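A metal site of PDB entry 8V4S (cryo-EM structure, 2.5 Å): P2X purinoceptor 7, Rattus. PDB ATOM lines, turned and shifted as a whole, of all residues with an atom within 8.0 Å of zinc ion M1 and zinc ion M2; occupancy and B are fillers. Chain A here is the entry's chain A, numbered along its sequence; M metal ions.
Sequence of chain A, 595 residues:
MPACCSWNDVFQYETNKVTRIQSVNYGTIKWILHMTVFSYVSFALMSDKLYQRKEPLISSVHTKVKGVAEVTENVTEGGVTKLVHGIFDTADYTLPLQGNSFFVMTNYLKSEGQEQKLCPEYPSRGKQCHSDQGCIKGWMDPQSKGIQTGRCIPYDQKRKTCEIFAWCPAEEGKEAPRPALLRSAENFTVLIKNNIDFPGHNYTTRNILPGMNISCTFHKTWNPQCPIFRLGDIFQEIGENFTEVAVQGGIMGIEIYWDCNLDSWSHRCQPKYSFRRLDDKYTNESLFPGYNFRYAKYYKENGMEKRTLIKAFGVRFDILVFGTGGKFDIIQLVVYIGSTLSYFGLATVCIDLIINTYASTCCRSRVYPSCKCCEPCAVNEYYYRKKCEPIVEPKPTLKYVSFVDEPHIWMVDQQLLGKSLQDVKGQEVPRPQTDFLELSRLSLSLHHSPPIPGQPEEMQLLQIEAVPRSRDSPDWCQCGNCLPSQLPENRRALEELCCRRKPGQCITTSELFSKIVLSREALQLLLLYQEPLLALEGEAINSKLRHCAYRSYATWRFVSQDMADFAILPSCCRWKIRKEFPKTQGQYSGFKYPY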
ATOM      1  N   VAL A 404     -29.109   6.382  20.009  1.00  0.00           N
ATOM      2  CA  VAL A 404     -28.830   6.622  21.418  1.00  0.00           C
ATOM      3  C   VAL A 404     -27.931   7.828  21.605  1.00  0.00           C
ATOM      4  O   VAL A 404     -27.979   8.500  22.645  1.00  0.00           O
ATOM      5  CB  VAL A 404     -28.226   5.349  22.071  1.00  0.00           C
ATOM      6  CG1 VAL A 404     -26.815   5.097  21.557  1.00  0.00           C
ATOM      7  CG2 VAL A 404     -28.242   5.473  23.582  1.00  0.00           C
ATOM      8  N   GLN A 422     -29.387   3.330   7.547  1.00  0.00           N
ATOM      9  CA  GLN A 422     -28.555   4.160   8.395  1.00  0.00           C
ATOM     10  C   GLN A 422     -28.240   5.505   7.739  1.00  0.00           C
ATOM     11  O   GLN A 422     -28.288   6.552   8.402  1.00  0.00           O
ATOM     12  CB  GLN A 422     -27.258   3.423   8.729  1.00  0.00           C
ATOM     13  CG  GLN A 422     -26.348   4.169   9.693  1.00  0.00           C
ATOM     14  CD  GLN A 422     -26.763   3.985  11.130  1.00  0.00           C
ATOM     15  OE1 GLN A 422     -27.679   3.225  11.436  1.00  0.00           O
ATOM     16  NE2 GLN A 422     -26.084   4.678  12.034  1.00  0.00           N
ATOM     17  N   SER A 473     -17.343  -5.646  12.072  1.00  0.00           N
ATOM     18  CA  SER A 473     -18.626  -4.971  12.051  1.00  0.00           C
ATOM     19  C   SER A 473     -18.904  -4.383  10.672  1.00  0.00           C
ATOM     20  O   SER A 473     -17.974  -4.055   9.927  1.00  0.00           O
ATOM     21  CB  SER A 473     -18.670  -3.865  13.107  1.00  0.00           C
ATOM     22  OG  SER A 473     -17.733  -2.848  12.811  1.00  0.00           O
ATOM     23  N   PRO A 474     -20.174  -4.245  10.300  1.00  0.00           N
ATOM     24  CA  PRO A 474     -20.500  -3.665   8.983  1.00  0.00           C
ATOM     25  C   PRO A 474     -20.040  -2.220   8.880  1.00  0.00           C
ATOM     26  O   PRO A 474     -19.729  -1.560   9.870  1.00  0.00           O
ATOM     27  CB  PRO A 474     -22.030  -3.765   8.923  1.00  0.00           C
ATOM     28  CG  PRO A 474     -22.382  -4.850   9.884  1.00  0.00           C
ATOM     29  CD  PRO A 474     -21.373  -4.751  10.987  1.00  0.00           C
ATOM     30  N   TRP A 476     -21.768   0.357   8.010  1.00  0.00           N
ATOM     31  CA  TRP A 476     -22.760   1.261   8.576  1.00  0.00           C
ATOM     32  C   TRP A 476     -22.931   1.114  10.077  1.00  0.00           C
ATOM     33  O   TRP A 476     -23.784   1.783  10.665  1.00  0.00           O
ATOM     34  CB  TRP A 476     -24.112   1.056   7.884  1.00  0.00           C
ATOM     35  CG  TRP A 476     -24.476  -0.389   7.689  1.00  0.00           C
ATOM     36  CD1 TRP A 476     -24.352  -1.111   6.535  1.00  0.00           C
ATOM     37  CD2 TRP A 476     -25.019  -1.280   8.659  1.00  0.00           C
ATOM     38  NE1 TRP A 476     -24.784  -2.398   6.734  1.00  0.00           N
ATOM     39  CE2 TRP A 476     -25.204  -2.526   8.038  1.00  0.00           C
ATOM     40  CE3 TRP A 476     -25.377  -1.145  10.008  1.00  0.00           C
ATOM     41  CZ2 TRP A 476     -25.728  -3.626   8.702  1.00  0.00           C
ATOM     42  CZ3 TRP A 476     -25.893  -2.239  10.671  1.00  0.00           C
ATOM     43  CH2 TRP A 476     -26.062  -3.464  10.017  1.00  0.00           C
ATOM     44  N   CYS A 477     -22.150   0.237  10.720  1.00  0.00           N
ATOM     45  CA  CYS A 477     -22.256   0.001  12.152  1.00  0.00           C
ATOM     46  C   CYS A 477     -21.218   0.830  12.889  1.00  0.00           C
ATOM     47  O   CYS A 477     -20.015   0.691  12.638  1.00  0.00           O
ATOM     48  CB  CYS A 477     -22.076  -1.482  12.466  1.00  0.00           C
ATOM     49  SG  CYS A 477     -21.953  -1.825  14.240  1.00  0.00           S
ATOM     50  N   GLN A 478     -21.676   1.691  13.791  1.00  0.00           N
ATOM     51  CA  GLN A 478     -20.812   2.537  14.604  1.00  0.00           C
ATOM     52  C   GLN A 478     -20.692   2.038  16.044  1.00  0.00           C
ATOM     53  O   GLN A 478     -20.135   2.738  16.888  1.00  0.00           O
ATOM     54  CB  GLN A 478     -21.309   3.971  14.589  1.00  0.00           C
ATOM     55  CG  GLN A 478     -20.761   4.822  13.449  1.00  0.00           C
ATOM     56  CD  GLN A 478     -21.578   4.679  12.171  1.00  0.00           C
ATOM     57  OE1 GLN A 478     -21.890   3.573  11.737  1.00  0.00           O
ATOM     58  NE2 GLN A 478     -21.921   5.811  11.562  1.00  0.00           N
ATOM     59  N   CYS A 479     -21.222   0.841  16.349  1.00  0.00           N
ATOM     60  CA  CYS A 479     -21.132   0.278  17.684  1.00  0.00           C
ATOM     61  C   CYS A 479     -20.376  -1.030  17.750  1.00  0.00           C
ATOM     62  O   CYS A 479     -19.871  -1.372  18.824  1.00  0.00           O
ATOM     63  CB  CYS A 479     -22.534   0.083  18.280  1.00  0.00           C
ATOM     64  SG  CYS A 479     -23.498  -1.277  17.577  1.00  0.00           S
ATOM     65  N   GLY A 480     -20.291  -1.788  16.653  1.00  0.00           N
ATOM     66  CA  GLY A 480     -19.511  -3.006  16.610  1.00  0.00           C
ATOM     67  C   GLY A 480     -20.288  -4.272  16.908  1.00  0.00           C
ATOM     68  O   GLY A 480     -19.809  -5.356  16.555  1.00  0.00           O
ATOM     69  N   ASN A 481     -21.455  -4.174  17.541  1.00  0.00           N
ATOM     70  CA  ASN A 481     -22.248  -5.356  17.854  1.00  0.00           C
ATOM     71  C   ASN A 481     -23.267  -5.689  16.770  1.00  0.00           C
ATOM     72  O   ASN A 481     -23.912  -6.734  16.855  1.00  0.00           O
ATOM     73  CB  ASN A 481     -22.965  -5.160  19.198  1.00  0.00           C
ATOM     74  CG  ASN A 481     -23.374  -6.476  19.839  1.00  0.00           C
ATOM     75  OD1 ASN A 481     -24.488  -6.954  19.631  1.00  0.00           O
ATOM     76  ND2 ASN A 481     -22.469  -7.069  20.608  1.00  0.00           N
ATOM     77  N   CYS A 482     -23.416  -4.834  15.762  1.00  0.00           N
ATOM     78  CA  CYS A 482     -24.369  -5.100  14.696  1.00  0.00           C
ATOM     79  C   CYS A 482     -23.871  -6.237  13.806  1.00  0.00           C
ATOM     80  O   CYS A 482     -22.665  -6.491  13.700  1.00  0.00           O
ATOM     81  CB  CYS A 482     -24.593  -3.844  13.856  1.00  0.00           C
ATOM     82  SG  CYS A 482     -25.614  -2.580  14.644  1.00  0.00           S
ATOM     83  N   LEU A 483     -24.816  -6.922  13.172  1.00  0.00           N
ATOM     84  CA  LEU A 483     -24.525  -8.047  12.299  1.00  0.00           C
ATOM     85  C   LEU A 483     -25.178  -7.853  10.946  1.00  0.00           C
ATOM     86  O   LEU A 483     -26.196  -7.164  10.838  1.00  0.00           O
ATOM     87  CB  LEU A 483     -25.007  -9.361  12.914  1.00  0.00           C
ATOM     88  CG  LEU A 483     -24.444  -9.758  14.276  1.00  0.00           C
ATOM     89  CD1 LEU A 483     -24.937 -11.134  14.680  1.00  0.00           C
ATOM     90  CD2 LEU A 483     -22.923  -9.707  14.277  1.00  0.00           C
ATOM     91  N   LEU A 497     -29.356  -0.914   9.999  1.00  0.00           N
ATOM     92  CA  LEU A 497     -29.471   0.252  10.871  1.00  0.00           C
ATOM     93  C   LEU A 497     -28.643   0.020  12.126  1.00  0.00           C
ATOM     94  O   LEU A 497     -28.585  -1.092  12.647  1.00  0.00           O
ATOM     95  CB  LEU A 497     -30.935   0.521  11.245  1.00  0.00           C
ATOM     96  CG  LEU A 497     -31.238   1.763  12.090  1.00  0.00           C
ATOM     97  CD1 LEU A 497     -31.040   3.029  11.282  1.00  0.00           C
ATOM     98  CD2 LEU A 497     -32.654   1.686  12.645  1.00  0.00           C
ATOM     99  N   CYS A 498     -28.011   1.087  12.610  1.00  0.00           N
ATOM    100  CA  CYS A 498     -27.190   1.038  13.812  1.00  0.00           C
ATOM    101  C   CYS A 498     -27.860   1.846  14.917  1.00  0.00           C
ATOM    102  O   CYS A 498     -28.699   2.715  14.664  1.00  0.00           O
ATOM    103  CB  CYS A 498     -25.773   1.564  13.557  1.00  0.00           C
ATOM    104  SG  CYS A 498     -24.540   1.051  14.772  1.00  0.00           S
ATOM    105  N   CYS A 499     -27.464   1.573  16.156  1.00  0.00           N
ATOM    106  CA  CYS A 499     -28.039   2.233  17.313  1.00  0.00           C
ATOM    107  C   CYS A 499     -27.517   3.650  17.507  1.00  0.00           C
ATOM    108  O   CYS A 499     -28.089   4.393  18.319  1.00  0.00           O
ATOM    109  CB  CYS A 499     -27.774   1.420  18.580  1.00  0.00           C
ATOM    110  SG  CYS A 499     -26.033   1.148  18.943  1.00  0.00           S
ATOM    111  N   ARG A 500     -26.450   4.031  16.814  1.00  0.00           N
ATOM    112  CA  ARG A 500     -25.846   5.345  16.977  1.00  0.00           C
ATOM    113  C   ARG A 500     -25.314   5.831  15.639  1.00  0.00           C
ATOM    114  O   ARG A 500     -24.933   5.025  14.786  1.00  0.00           O
ATOM    115  CB  ARG A 500     -24.731   5.322  18.021  1.00  0.00           C
ATOM    116  CG  ARG A 500     -23.920   4.029  18.011  1.00  0.00           C
ATOM    117  CD  ARG A 500     -22.738   4.069  18.978  1.00  0.00           C
ATOM    118  NE  ARG A 500     -23.065   4.639  20.277  1.00  0.00           N
ATOM    119  CZ  ARG A 500     -22.720   5.867  20.660  1.00  0.00           C
ATOM    120  NH1 ARG A 500     -22.035   6.653  19.841  1.00  0.00           N
ATOM    121  NH2 ARG A 500     -23.061   6.309  21.862  1.00  0.00           N
ATOM    122  N   GLY A 504     -19.000   4.752  19.271  1.00  0.00           N
ATOM    123  CA  GLY A 504     -19.111   4.805  20.720  1.00  0.00           C
ATOM    124  C   GLY A 504     -19.652   3.497  21.260  1.00  0.00           C
ATOM    125  O   GLY A 504     -19.637   2.473  20.585  1.00  0.00           O
ATOM    126  N   GLN A 505     -20.122   3.556  22.506  1.00  0.00           N
ATOM    127  CA  GLN A 505     -20.670   2.391  23.165  1.00  0.00           C
ATOM    128  C   GLN A 505     -22.034   2.020  22.582  1.00  0.00           C
ATOM    129  O   GLN A 505     -22.756   2.870  22.063  1.00  0.00           O
ATOM    130  CB  GLN A 505     -20.793   2.624  24.670  1.00  0.00           C
ATOM    131  CG  GLN A 505     -21.232   4.035  25.032  1.00  0.00           C
ATOM    132  CD  GLN A 505     -21.285   4.262  26.528  1.00  0.00           C
ATOM    133  OE1 GLN A 505     -21.527   3.337  27.307  1.00  0.00           O
ATOM    134  NE2 GLN A 505     -21.064   5.502  26.946  1.00  0.00           N
ATOM    135  N   CYS A 506     -22.369   0.737  22.666  1.00  0.00           N
ATOM    136  CA  CYS A 506     -23.628   0.242  22.148  1.00  0.00           C
ATOM    137  C   CYS A 506     -24.735   0.368  23.189  1.00  0.00           C
ATOM    138  O   CYS A 506     -24.470   0.383  24.401  1.00  0.00           O
ATOM    139  CB  CYS A 506     -23.498  -1.227  21.713  1.00  0.00           C
ATOM    140  SG  CYS A 506     -24.988  -1.927  20.995  1.00  0.00           S
ATOM    141  N   ILE A 507     -25.970   0.475  22.714  1.00  0.00           N
ATOM    142  CA  ILE A 507     -27.120   0.557  23.595  1.00  0.00           C
ATOM    143  C   ILE A 507     -27.289  -0.730  24.389  1.00  0.00           C
ATOM    144  O   ILE A 507     -27.702  -0.708  25.554  1.00  0.00           O
ATOM    145  CB  ILE A 507     -28.388   0.899  22.792  1.00  0.00           C
ATOM    146  CG1 ILE A 507     -29.628   0.933  23.683  1.00  0.00           C
ATOM    147  CG2 ILE A 507     -28.578  -0.073  21.656  1.00  0.00           C
ATOM    148  CD1 ILE A 507     -29.799   2.220  24.437  1.00  0.00           C
ATOM    149  N   THR A 508     -26.972  -1.877  23.785  1.00  0.00           N
ATOM    150  CA  THR A 508     -27.149  -3.167  24.443  1.00  0.00           C
ATOM    151  C   THR A 508     -26.255  -3.328  25.665  1.00  0.00           C
ATOM    152  O   THR A 508     -26.536  -4.179  26.507  1.00  0.00           O
ATOM    153  CB  THR A 508     -26.889  -4.309  23.460  1.00  0.00           C
ATOM    154  OG1 THR A 508     -25.572  -4.163  22.902  1.00  0.00           O
ATOM    155  CG2 THR A 508     -27.914  -4.298  22.345  1.00  0.00           C
ATOM    156  N   THR A 509     -25.185  -2.539  25.777  1.00  0.00           N
ATOM    157  CA  THR A 509     -24.269  -2.669  26.902  1.00  0.00           C
ATOM    158  C   THR A 509     -24.890  -2.202  28.210  1.00  0.00           C
ATOM    159  O   THR A 509     -24.439  -2.622  29.277  1.00  0.00           O
ATOM    160  CB  THR A 509     -22.981  -1.885  26.639  1.00  0.00           C
ATOM    161  OG1 THR A 509     -23.273  -0.481  26.591  1.00  0.00           O
ATOM    162  CG2 THR A 509     -22.368  -2.315  25.305  1.00  0.00           C
ATOM    163  N   TYR A 553     -38.582  -2.924  23.424  1.00  0.00           N
ATOM    164  CA  TYR A 553     -37.557  -1.978  22.982  1.00  0.00           C
ATOM    165  C   TYR A 553     -38.185  -0.799  22.256  1.00  0.00           C
ATOM    166  O   TYR A 553     -37.790   0.351  22.471  1.00  0.00           O
ATOM    167  CB  TYR A 553     -36.534  -2.676  22.080  1.00  0.00           C
ATOM    168  CG  TYR A 553     -35.482  -1.716  21.552  1.00  0.00           C
ATOM    169  CD1 TYR A 553     -34.338  -1.447  22.279  1.00  0.00           C
ATOM    170  CD2 TYR A 553     -35.642  -1.079  20.331  1.00  0.00           C
ATOM    171  CE1 TYR A 553     -33.382  -0.568  21.804  1.00  0.00           C
ATOM    172  CE2 TYR A 553     -34.695  -0.205  19.844  1.00  0.00           C
ATOM    173  CZ  TYR A 553     -33.564   0.051  20.587  1.00  0.00           C
ATOM    174  OH  TYR A 553     -32.614   0.924  20.114  1.00  0.00           O
ATOM    175  N   PRO A 570     -32.447  -1.454  15.582  1.00  0.00           N
ATOM    176  CA  PRO A 570     -31.105  -1.603  15.017  1.00  0.00           C
ATOM    177  C   PRO A 570     -30.645  -3.056  15.031  1.00  0.00           C
ATOM    178  O   PRO A 570     -31.194  -3.900  15.737  1.00  0.00           O
ATOM    179  CB  PRO A 570     -30.230  -0.734  15.930  1.00  0.00           C
ATOM    180  CG  PRO A 570     -31.002  -0.599  17.181  1.00  0.00           C
ATOM    181  CD  PRO A 570     -32.450  -0.642  16.809  1.00  0.00           C
ATOM    182  N   SER A 571     -29.632  -3.337  14.212  1.00  0.00           N
ATOM    183  CA  SER A 571     -29.192  -4.714  14.026  1.00  0.00           C
ATOM    184  C   SER A 571     -28.645  -5.311  15.308  1.00  0.00           C
ATOM    185  O   SER A 571     -28.854  -6.500  15.587  1.00  0.00           O
ATOM    186  CB  SER A 571     -28.147  -4.781  12.914  1.00  0.00           C
ATOM    187  OG  SER A 571     -28.735  -4.537  11.650  1.00  0.00           O
ATOM    188  N   CYS A 572     -27.930  -4.509  16.108  1.00  0.00           N
ATOM    189  CA  CYS A 572     -27.350  -5.031  17.344  1.00  0.00           C
ATOM    190  C   CYS A 572     -28.428  -5.530  18.301  1.00  0.00           C
ATOM    191  O   CYS A 572     -28.359  -6.662  18.790  1.00  0.00           O
ATOM    192  CB  CYS A 572     -26.493  -3.942  18.005  1.00  0.00           C
ATOM    193  SG  CYS A 572     -27.225  -2.298  17.973  1.00  0.00           S
ATOM    194  N   CYS A 573     -29.433  -4.686  18.569  1.00  0.00           N
ATOM    195  CA  CYS A 573     -30.515  -5.088  19.453  1.00  0.00           C
ATOM    196  C   CYS A 573     -31.294  -6.264  18.886  1.00  0.00           C
ATOM    197  O   CYS A 573     -31.635  -7.210  19.606  1.00  0.00           O
ATOM    198  CB  CYS A 573     -31.462  -3.914  19.697  1.00  0.00           C
ATOM    199  SG  CYS A 573     -30.641  -2.406  20.222  1.00  0.00           S
HETATM  200 ZN    ZN M   1     -23.910  -1.134  15.297  1.00  0.00          ZN
HETATM  201 ZN    ZN M   2     -25.431  -1.095  18.869  1.00  0.00          ZN
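The backbone NH (N) of Gln 478 lies close to the side-chain sulfur (SG) of Cys 498 (3.1 Å). The backbone NH (N) of Asn 481 sits close to the side-chain sulfur (SG) of Cys 479, 3.5 Å away. O of Cys 506 sits at hydrogen-bond distance from OG1 of Thr 509, 2.6 Å away. SG of Cys 482 sits close to N of Cys 572 (3.4 Å). The side-chain sulfur (SG) of Cys 506 lies close to the side-chain hydroxyl (OG1) of Thr 508, 3.0 Å away. The backbone carbonyl oxygen (O) of Trp 476 lies close to the side-chain amide oxygen (OE1) of Gln 478 (2.8 Å). N of Gly 480 lies close to SG of Cys 477 (2.9 Å). OE1 of Gln 422 sits at hydrogen-bond distance from N of Cys 498 (2.5 Å).
Residues that only touch zinc ion M1: Gln 478 (3.9 Å) and Gly 480 (3.9 Å). The nearest printed residue that does not touch zinc ion M1 is Cys 572 (4.4 Å).
Along chain A the residues within 4 Å of zinc ion M2 span positions 479 to 572.
Zinc ion M1 is bound by SG of Cys 479 (2.3 Å), SG of Cys 482 (2.3 Å), SG of Cys 477 (2.3 Å) and SG of Cys 498 (2.3 Å). Zinc ion M1 has four donor atoms within binding distance.
Zinc ion M2 is bound by SG of Cys 499, SG of Cys 506, SG of Cys 479 and SG of Cys 572. Zinc ion M2 has four donor atoms within binding distance.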
